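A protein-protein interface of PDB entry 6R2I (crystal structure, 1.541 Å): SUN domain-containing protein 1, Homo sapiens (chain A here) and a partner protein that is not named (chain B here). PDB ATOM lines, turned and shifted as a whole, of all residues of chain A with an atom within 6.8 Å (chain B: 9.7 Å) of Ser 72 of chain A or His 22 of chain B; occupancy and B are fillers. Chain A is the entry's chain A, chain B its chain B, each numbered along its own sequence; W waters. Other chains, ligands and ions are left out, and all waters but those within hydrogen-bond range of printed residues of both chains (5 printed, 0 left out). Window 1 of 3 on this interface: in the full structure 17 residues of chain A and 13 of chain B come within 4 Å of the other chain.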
ATOM      1  N   ILE A  43      23.118  -1.142  -7.882  1.00  0.00           N
ATOM      2  CA  ILE A  43      22.671  -1.552  -6.554  1.00  0.00           C
ATOM      3  C   ILE A  43      22.573  -3.072  -6.482  1.00  0.00           C
ATOM      4  O   ILE A  43      21.962  -3.715  -7.358  1.00  0.00           O
ATOM      5  CB  ILE A  43      21.309  -0.927  -6.221  1.00  0.00           C
ATOM      6  CG1 ILE A  43      21.356   0.600  -6.262  1.00  0.00           C
ATOM      7  CG2 ILE A  43      20.808  -1.454  -4.853  1.00  0.00           C
ATOM      8  CD1 ILE A  43      22.329   1.222  -5.312  1.00  0.00           C
ATOM      9  N   SER A  45      20.486  -5.407  -4.924  1.00  0.00           N
ATOM     10  CA  SER A  45      19.168  -5.190  -4.312  1.00  0.00           C
ATOM     11  C   SER A  45      18.901  -6.114  -3.120  1.00  0.00           C
ATOM     12  O   SER A  45      18.289  -5.695  -2.129  1.00  0.00           O
ATOM     13  CB  SER A  45      18.067  -5.386  -5.364  1.00  0.00           C
ATOM     14  OG  SER A  45      18.216  -4.422  -6.393  1.00  0.00           O
ATOM     15  N   THR A  51      12.496  -0.771   1.842  1.00  0.00           N
ATOM     16  CA  THR A  51      12.056   0.581   1.558  1.00  0.00           C
ATOM     17  C   THR A  51      10.881   0.963   2.439  1.00  0.00           C
ATOM     18  O   THR A  51       9.993   0.136   2.733  1.00  0.00           O
ATOM     19  CB  THR A  51      11.674   0.709   0.086  1.00  0.00           C
ATOM     20  OG1 THR A  51      12.818   0.383  -0.719  1.00  0.00           O
ATOM     21  CG2 THR A  51      11.198   2.128  -0.251  1.00  0.00           C
ATOM     22  N   PHE A  69       3.574   4.461  -6.374  1.00  0.00           N
ATOM     23  CA  PHE A  69       4.970   4.725  -6.704  1.00  0.00           C
ATOM     24  C   PHE A  69       5.744   5.148  -5.459  1.00  0.00           C
ATOM     25  O   PHE A  69       5.262   5.952  -4.659  1.00  0.00           O
ATOM     26  CB  PHE A  69       5.086   5.832  -7.797  1.00  0.00           C
ATOM     27  CG  PHE A  69       6.496   6.285  -8.061  1.00  0.00           C
ATOM     28  CD1 PHE A  69       7.331   5.543  -8.882  1.00  0.00           C
ATOM     29  CD2 PHE A  69       6.987   7.446  -7.489  1.00  0.00           C
ATOM     30  CE1 PHE A  69       8.631   5.937  -9.122  1.00  0.00           C
ATOM     31  CE2 PHE A  69       8.305   7.857  -7.729  1.00  0.00           C
ATOM     32  CZ  PHE A  69       9.122   7.098  -8.545  1.00  0.00           C
ATOM     33  N   SER A  70       6.948   4.604  -5.303  1.00  0.00           N
ATOM     34  CA  SER A  70       7.912   5.099  -4.320  1.00  0.00           C
ATOM     35  C   SER A  70       9.317   4.992  -4.904  1.00  0.00           C
ATOM     36  O   SER A  70       9.584   4.165  -5.762  1.00  0.00           O
ATOM     37  CB  SER A  70       7.836   4.296  -3.027  1.00  0.00           C
ATOM     38  OG  SER A  70       8.180   2.951  -3.282  1.00  0.00           O
ATOM     39  N   GLN A  71      10.238   5.828  -4.432  1.00  0.00           N
ATOM     40  CA  GLN A  71      11.575   5.810  -5.001  1.00  0.00           C
ATOM     41  C   GLN A  71      12.332   4.548  -4.599  1.00  0.00           C
ATOM     42  O   GLN A  71      12.240   4.087  -3.457  1.00  0.00           O
ATOM     43  CB  GLN A  71      12.364   7.027  -4.526  1.00  0.00           C
ATOM     44  CG  GLN A  71      11.706   8.368  -4.779  1.00  0.00           C
ATOM     45  CD  GLN A  71      11.891   8.888  -6.179  1.00  0.00           C
ATOM     46  OE1 GLN A  71      12.403   8.200  -7.059  1.00  0.00           O
ATOM     47  NE2 GLN A  71      11.477  10.139  -6.398  1.00  0.00           N
ATOM     48  N   SER A  72      13.130   4.024  -5.512  1.00  0.00           N
ATOM     49  CA  SER A  72      13.948   2.851  -5.224  1.00  0.00           C
ATOM     50  C   SER A  72      15.370   3.241  -4.827  1.00  0.00           C
ATOM     51  O   SER A  72      15.800   4.391  -5.006  1.00  0.00           O
ATOM     52  CB  SER A  72      13.955   1.915  -6.426  1.00  0.00           C
ATOM     53  OG  SER A  72      15.111   1.976  -7.203  1.00  0.00           O
ATOM     54  N   PRO A  73      16.146   2.291  -4.293  1.00  0.00           N
ATOM     55  CA  PRO A  73      17.546   2.601  -3.909  1.00  0.00           C
ATOM     56  C   PRO A  73      18.423   3.038  -5.071  1.00  0.00           C
ATOM     57  O   PRO A  73      19.454   3.694  -4.831  1.00  0.00           O
ATOM     58  CB  PRO A  73      18.045   1.287  -3.282  1.00  0.00           C
ATOM     59  CG  PRO A  73      16.884   0.385  -3.225  1.00  0.00           C
ATOM     60  CD  PRO A  73      15.768   0.898  -4.012  1.00  0.00           C
ATOM     61  N   ARG A  74      18.034   2.752  -6.318  1.00  0.00           N
ATOM     62  CA  ARG A  74      18.775   3.215  -7.491  1.00  0.00           C
ATOM     63  C   ARG A  74      18.937   4.733  -7.520  1.00  0.00           C
ATOM     64  O   ARG A  74      19.927   5.227  -8.068  1.00  0.00           O
ATOM     65  CB  ARG A  74      18.095   2.745  -8.786  1.00  0.00           C
ATOM     66  CG  ARG A  74      18.147   1.226  -9.047  1.00  0.00           C
ATOM     67  CD  ARG A  74      17.337   0.820 -10.283  1.00  0.00           C
ATOM     68  NE  ARG A  74      17.863   1.491 -11.462  1.00  0.00           N
ATOM     69  CZ  ARG A  74      17.222   1.700 -12.606  1.00  0.00           C
ATOM     70  NH1 ARG A  74      15.975   1.261 -12.821  1.00  0.00           N
ATOM     71  NH2 ARG A  74      17.857   2.377 -13.555  1.00  0.00           N
ATOM     72  N   VAL A  75      17.998   5.496  -6.940  1.00  0.00           N
ATOM     73  CA  VAL A  75      18.118   6.959  -7.035  1.00  0.00           C
ATOM     74  C   VAL A  75      19.322   7.471  -6.251  1.00  0.00           C
ATOM     75  O   VAL A  75      19.809   8.593  -6.519  1.00  0.00           O
ATOM     76  CB  VAL A  75      16.852   7.735  -6.579  1.00  0.00           C
ATOM     77  CG1 VAL A  75      15.643   7.380  -7.417  1.00  0.00           C
ATOM     78  CG2 VAL A  75      16.592   7.652  -5.063  1.00  0.00           C
ATOM     79  N   VAL A  76      19.849   6.677  -5.305  1.00  0.00           N
ATOM     80  CA  VAL A  76      21.014   7.118  -4.534  1.00  0.00           C
ATOM     81  C   VAL A  76      22.290   7.182  -5.388  1.00  0.00           C
ATOM     82  O   VAL A  76      23.270   7.846  -4.991  1.00  0.00           O
ATOM     83  CB  VAL A  76      21.206   6.200  -3.299  1.00  0.00           C
ATOM     84  CG1 VAL A  76      22.371   6.663  -2.451  1.00  0.00           C
ATOM     85  CG2 VAL A  76      19.977   6.112  -2.439  1.00  0.00           C
ATOM     86  N   GLN A  78      22.107   8.201  -8.719  1.00  0.00           N
ATOM     87  CA  GLN A  78      21.672   9.100  -9.796  1.00  0.00           C
ATOM     88  C   GLN A  78      21.780  10.560  -9.355  1.00  0.00           C
ATOM     89  O   GLN A  78      21.543  10.880  -8.175  1.00  0.00           O
ATOM     90  CB  GLN A  78      20.220   8.728 -10.224  1.00  0.00           C
ATOM     91  CG  GLN A  78      20.085   7.287 -10.718  1.00  0.00           C
ATOM     92  CD  GLN A  78      18.643   6.833 -10.953  1.00  0.00           C
ATOM     93  OE1 GLN A  78      17.690   7.545 -10.606  1.00  0.00           O
ATOM     94  NE2 GLN A  78      18.476   5.634 -11.528  1.00  0.00           N
ATOM     95  N   CYS A  86      15.118  10.966  -3.509  1.00  0.00           N
ATOM     96  CA  CYS A  86      15.865  10.328  -2.430  1.00  0.00           C
ATOM     97  C   CYS A  86      15.203   8.995  -2.101  1.00  0.00           C
ATOM     98  O   CYS A  86      13.994   8.812  -2.329  1.00  0.00           O
ATOM     99  CB  CYS A  86      15.919  11.205  -1.159  1.00  0.00           C
ATOM    100  SG  CYS A  86      14.295  11.830  -0.582  1.00  0.00           S
ATOM    101  N   TRP A  87      16.015   8.048  -1.610  1.00  0.00           N
ATOM    102  CA  TRP A  87      15.517   6.755  -1.136  1.00  0.00           C
ATOM    103  C   TRP A  87      15.259   6.824   0.368  1.00  0.00           C
ATOM    104  O   TRP A  87      16.144   7.223   1.134  1.00  0.00           O
ATOM    105  CB  TRP A  87      16.528   5.644  -1.452  1.00  0.00           C
ATOM    106  CG  TRP A  87      16.179   4.260  -0.905  1.00  0.00           C
ATOM    107  CD1 TRP A  87      15.060   3.536  -1.166  1.00  0.00           C
ATOM    108  CD2 TRP A  87      16.961   3.479   0.016  1.00  0.00           C
ATOM    109  NE1 TRP A  87      15.103   2.332  -0.490  1.00  0.00           N
ATOM    110  CE2 TRP A  87      16.260   2.263   0.238  1.00  0.00           C
ATOM    111  CE3 TRP A  87      18.189   3.676   0.651  1.00  0.00           C
ATOM    112  CZ2 TRP A  87      16.749   1.259   1.093  1.00  0.00           C
ATOM    113  CZ3 TRP A  87      18.686   2.669   1.482  1.00  0.00           C
ATOM    114  CH2 TRP A  87      17.960   1.483   1.700  1.00  0.00           C
ATOM    115  N   ALA A  88      14.085   6.365   0.802  1.00  0.00           N
ATOM    116  CA  ALA A  88      13.714   6.377   2.210  1.00  0.00           C
ATOM    117  C   ALA A  88      13.611   4.955   2.758  1.00  0.00           C
ATOM    118  O   ALA A  88      12.928   4.098   2.174  1.00  0.00           O
ATOM    119  CB  ALA A  88      12.381   7.091   2.426  1.00  0.00           C
ATOM    120  N   THR B  19       1.560  -1.913  -5.883  1.00  0.00           N
ATOM    121  CA  THR B  19       2.785  -1.123  -5.836  1.00  0.00           C
ATOM    122  C   THR B  19       3.662  -1.470  -7.032  1.00  0.00           C
ATOM    123  O   THR B  19       3.899  -2.650  -7.312  1.00  0.00           O
ATOM    124  CB  THR B  19       3.566  -1.376  -4.542  1.00  0.00           C
ATOM    125  OG1 THR B  19       2.862  -0.810  -3.430  1.00  0.00           O
ATOM    126  CG2 THR B  19       4.969  -0.767  -4.627  1.00  0.00           C
ATOM    127  N   TRP B  20       4.150  -0.450  -7.719  1.00  0.00           N
ATOM    128  CA  TRP B  20       5.033  -0.676  -8.851  1.00  0.00           C
ATOM    129  C   TRP B  20       6.351  -1.238  -8.347  1.00  0.00           C
ATOM    130  O   TRP B  20       7.123  -0.499  -7.724  1.00  0.00           O
ATOM    131  CB  TRP B  20       5.283   0.617  -9.618  1.00  0.00           C
ATOM    132  CG  TRP B  20       5.810   0.411 -11.019  1.00  0.00           C
ATOM    133  CD1 TRP B  20       5.309  -0.433 -11.968  1.00  0.00           C
ATOM    134  CD2 TRP B  20       6.925   1.080 -11.629  1.00  0.00           C
ATOM    135  NE1 TRP B  20       6.045  -0.340 -13.124  1.00  0.00           N
ATOM    136  CE2 TRP B  20       7.042   0.582 -12.944  1.00  0.00           C
ATOM    137  CE3 TRP B  20       7.836   2.048 -11.193  1.00  0.00           C
ATOM    138  CZ2 TRP B  20       8.032   1.018 -13.823  1.00  0.00           C
ATOM    139  CZ3 TRP B  20       8.820   2.478 -12.069  1.00  0.00           C
ATOM    140  CH2 TRP B  20       8.909   1.964 -13.368  1.00  0.00           C
ATOM    141  N   PRO B  21       6.654  -2.511  -8.579  1.00  0.00           N
ATOM    142  CA  PRO B  21       7.971  -3.018  -8.200  1.00  0.00           C
ATOM    143  C   PRO B  21       9.067  -2.129  -8.765  1.00  0.00           C
ATOM    144  O   PRO B  21       8.929  -1.541  -9.839  1.00  0.00           O
ATOM    145  CB  PRO B  21       8.005  -4.412  -8.829  1.00  0.00           C
ATOM    146  CG  PRO B  21       7.035  -4.294  -9.963  1.00  0.00           C
ATOM    147  CD  PRO B  21       5.926  -3.493  -9.398  1.00  0.00           C
ATOM    148  N   HIS B  22      10.157  -2.031  -8.024  1.00  0.00           N
ATOM    149  CA  HIS B  22      11.307  -1.270  -8.482  1.00  0.00           C
ATOM    150  C   HIS B  22      11.970  -2.014  -9.634  1.00  0.00           C
ATOM    151  O   HIS B  22      12.506  -3.113  -9.447  1.00  0.00           O
ATOM    152  CB  HIS B  22      12.271  -1.057  -7.321  1.00  0.00           C
ATOM    153  CG  HIS B  22      11.661  -0.331  -6.162  1.00  0.00           C
ATOM    154  ND1 HIS B  22      10.601   0.539  -6.305  1.00  0.00           N
ATOM    155  CD2 HIS B  22      11.963  -0.341  -4.842  1.00  0.00           C
ATOM    156  CE1 HIS B  22      10.276   1.031  -5.123  1.00  0.00           C
ATOM    157  NE2 HIS B  22      11.088   0.515  -4.218  1.00  0.00           N
ATOM    158  N   LEU B  23      11.903  -1.438 -10.835  1.00  0.00           N
ATOM    159  CA  LEU B  23      12.715  -1.918 -11.946  1.00  0.00           C
ATOM    160  C   LEU B  23      14.181  -1.965 -11.531  1.00  0.00           C
ATOM    161  O   LEU B  23      14.716  -0.993 -10.989  1.00  0.00           O
ATOM    162  CB  LEU B  23      12.545  -1.004 -13.161  1.00  0.00           C
ATOM    163  CG  LEU B  23      11.241  -1.072 -13.957  1.00  0.00           C
ATOM    164  CD1 LEU B  23      11.212   0.047 -14.988  1.00  0.00           C
ATOM    165  CD2 LEU B  23      11.094  -2.430 -14.627  1.00  0.00           C
ATOM    166  N   GLN B  24      14.828  -3.098 -11.787  1.00  0.00           N
ATOM    167  CA  GLN B  24      16.194  -3.336 -11.344  1.00  0.00           C
ATOM    168  C   GLN B  24      17.147  -3.376 -12.532  1.00  0.00           C
ATOM    169  O   GLN B  24      16.789  -3.825 -13.624  1.00  0.00           O
ATOM    170  CB  GLN B  24      16.284  -4.644 -10.559  1.00  0.00           C
ATOM    171  CG  GLN B  24      15.503  -4.618  -9.261  1.00  0.00           C
ATOM    172  CD  GLN B  24      15.430  -5.975  -8.598  1.00  0.00           C
ATOM    173  OE1 GLN B  24      15.483  -7.010  -9.265  1.00  0.00           O
ATOM    174  NE2 GLN B  24      15.312  -5.981  -7.277  1.00  0.00           N
ATOM    175  N   LEU B  25      18.372  -2.904 -12.302  1.00  0.00           N
ATOM    176  CA  LEU B  25      19.374  -2.763 -13.348  1.00  0.00           C
ATOM    177  C   LEU B  25      20.684  -3.374 -12.878  1.00  0.00           C
ATOM    178  O   LEU B  25      21.205  -2.988 -11.827  1.00  0.00           O
ATOM    179  CB  LEU B  25      19.586  -1.283 -13.709  1.00  0.00           C
ATOM    180  CG  LEU B  25      20.558  -0.958 -14.848  1.00  0.00           C
ATOM    181  CD1 LEU B  25      20.328   0.453 -15.384  1.00  0.00           C
ATOM    182  CD2 LEU B  25      22.008  -1.096 -14.403  1.00  0.00           C
HETATM  183  O   HOH W   1       7.125   2.023  -6.682  1.00  0.00           O
HETATM  184  O   HOH W   2      22.455  -5.077  -9.701  1.00  0.00           O
HETATM  185  O   HOH W   3      15.015  -0.787  -8.157  1.00  0.00           O
HETATM  186  O   HOH W   4      10.533   2.979  -8.279  1.00  0.00           O
HETATM  187  O   HOH W   5      21.308  -0.619 -10.159  1.00  0.00           O
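NE2 of Gln 24 of chain B sits close to OG of Ser 45 of chain A (3.4 Å).
NH1 of Arg 74 of chain A is in hydrogen-bond range of O of Leu 23 of chain B (3.2 Å).
The side-chain hydroxyl of Thr 51 of chain A lies within hydrogen-bond range of the indole nitrogen of Trp 87 of chain A (3.0 Å).
OG of Ser 72 of chain A lies close to N of Arg 74 of chain A (3.2 Å).
Thr 51 of chain A touches His 22 of chain B.
Ser 70 of chain A touches His 22 of chain B.
O of Gln 71 of chain A touches NE2 of His 22 of chain B, 3.8 Å away.
His 22 of chain B touches Ser 72 of chain A.
Leu 25 of chain B touches Arg 74 of chain A (CD1 to NH2, 3.6 Å).
Of chain B, only His 22 (3.2 Å) comes within 4 Å of Ser 72 of chain A.
His 22 of chain B touches just these residues of chain A: Thr 51, Ser 70, Gln 71 and Ser 72.
Ser 70 of chain A touches just one residue of chain B: His 22.
No residue of chain B comes within 4 Å of Pro 73 of chain A.
Printed residues of chain A within 4 Å of Leu 25 of chain B: Arg 74 (3.6 Å).
Of the printed residues of chain B, Gln 71 of chain A touches His 22 (3.8 Å).
Of the printed residues of chain A, Leu 23 of chain B touches Arg 74.
Printed residues of chain B within 4 Å of Thr 51 of chain A: His 22.
Of the printed residues of chain B, Ser 45 of chain A touches Gln 24 (3.4 Å).
Ile 43 of chain A touches none of the printed residues of chain B.
The nearest residue of chain B that does not touch Ser 72 of chain A is Leu 23 of chain B (4.8 Å).
The nearest residue of chain A that does not touch His 22 of chain B is Pro 73 of chain A (4.1 Å).
Of the 15 printed residues of chain A, 6 touch a printed residue of chain B.
Printed residues of chain A that touch a printed residue of chain B: Ser 45, Thr 51, Ser 70, Gln 71, Ser 72 and Arg 74.
Of the 7 printed residues of chain B, 4 touch a printed residue of chain A.
Hydrophobic or aromatic side chains of chain B that line the printed part of chain A: His 22 and Leu 25.
Among the printed residues, no Asp or Glu carboxylate lies within 4 Å of a Lys or Arg side-chain nitrogen of the other chain.
Water W1 bridges O of Trp 20 of chain B (2.7 Å) and N of Ser 70 of chain A (2.9 Å).
Water W2 bridges the backbone carbonyl oxygen (O) of Ile 43 of chain A and the backbone carbonyl oxygen (O) of Leu 25 of chain B.
Water W3 bridges the backbone carbonyl oxygen (O) of Leu 23 of chain B and the side-chain hydroxyl (OG) of Ser 72 of chain A.
Water W5 lies within hydrogen-bond range of O of Leu 25 of chain B (2.9 Å) and N of Ile 43 of chain A (3.0 Å).
Water W4 lies within hydrogen-bond range of O of Ser 70 of chain A (2.9 Å) and ND1 of His 22 of chain B (3.1 Å).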
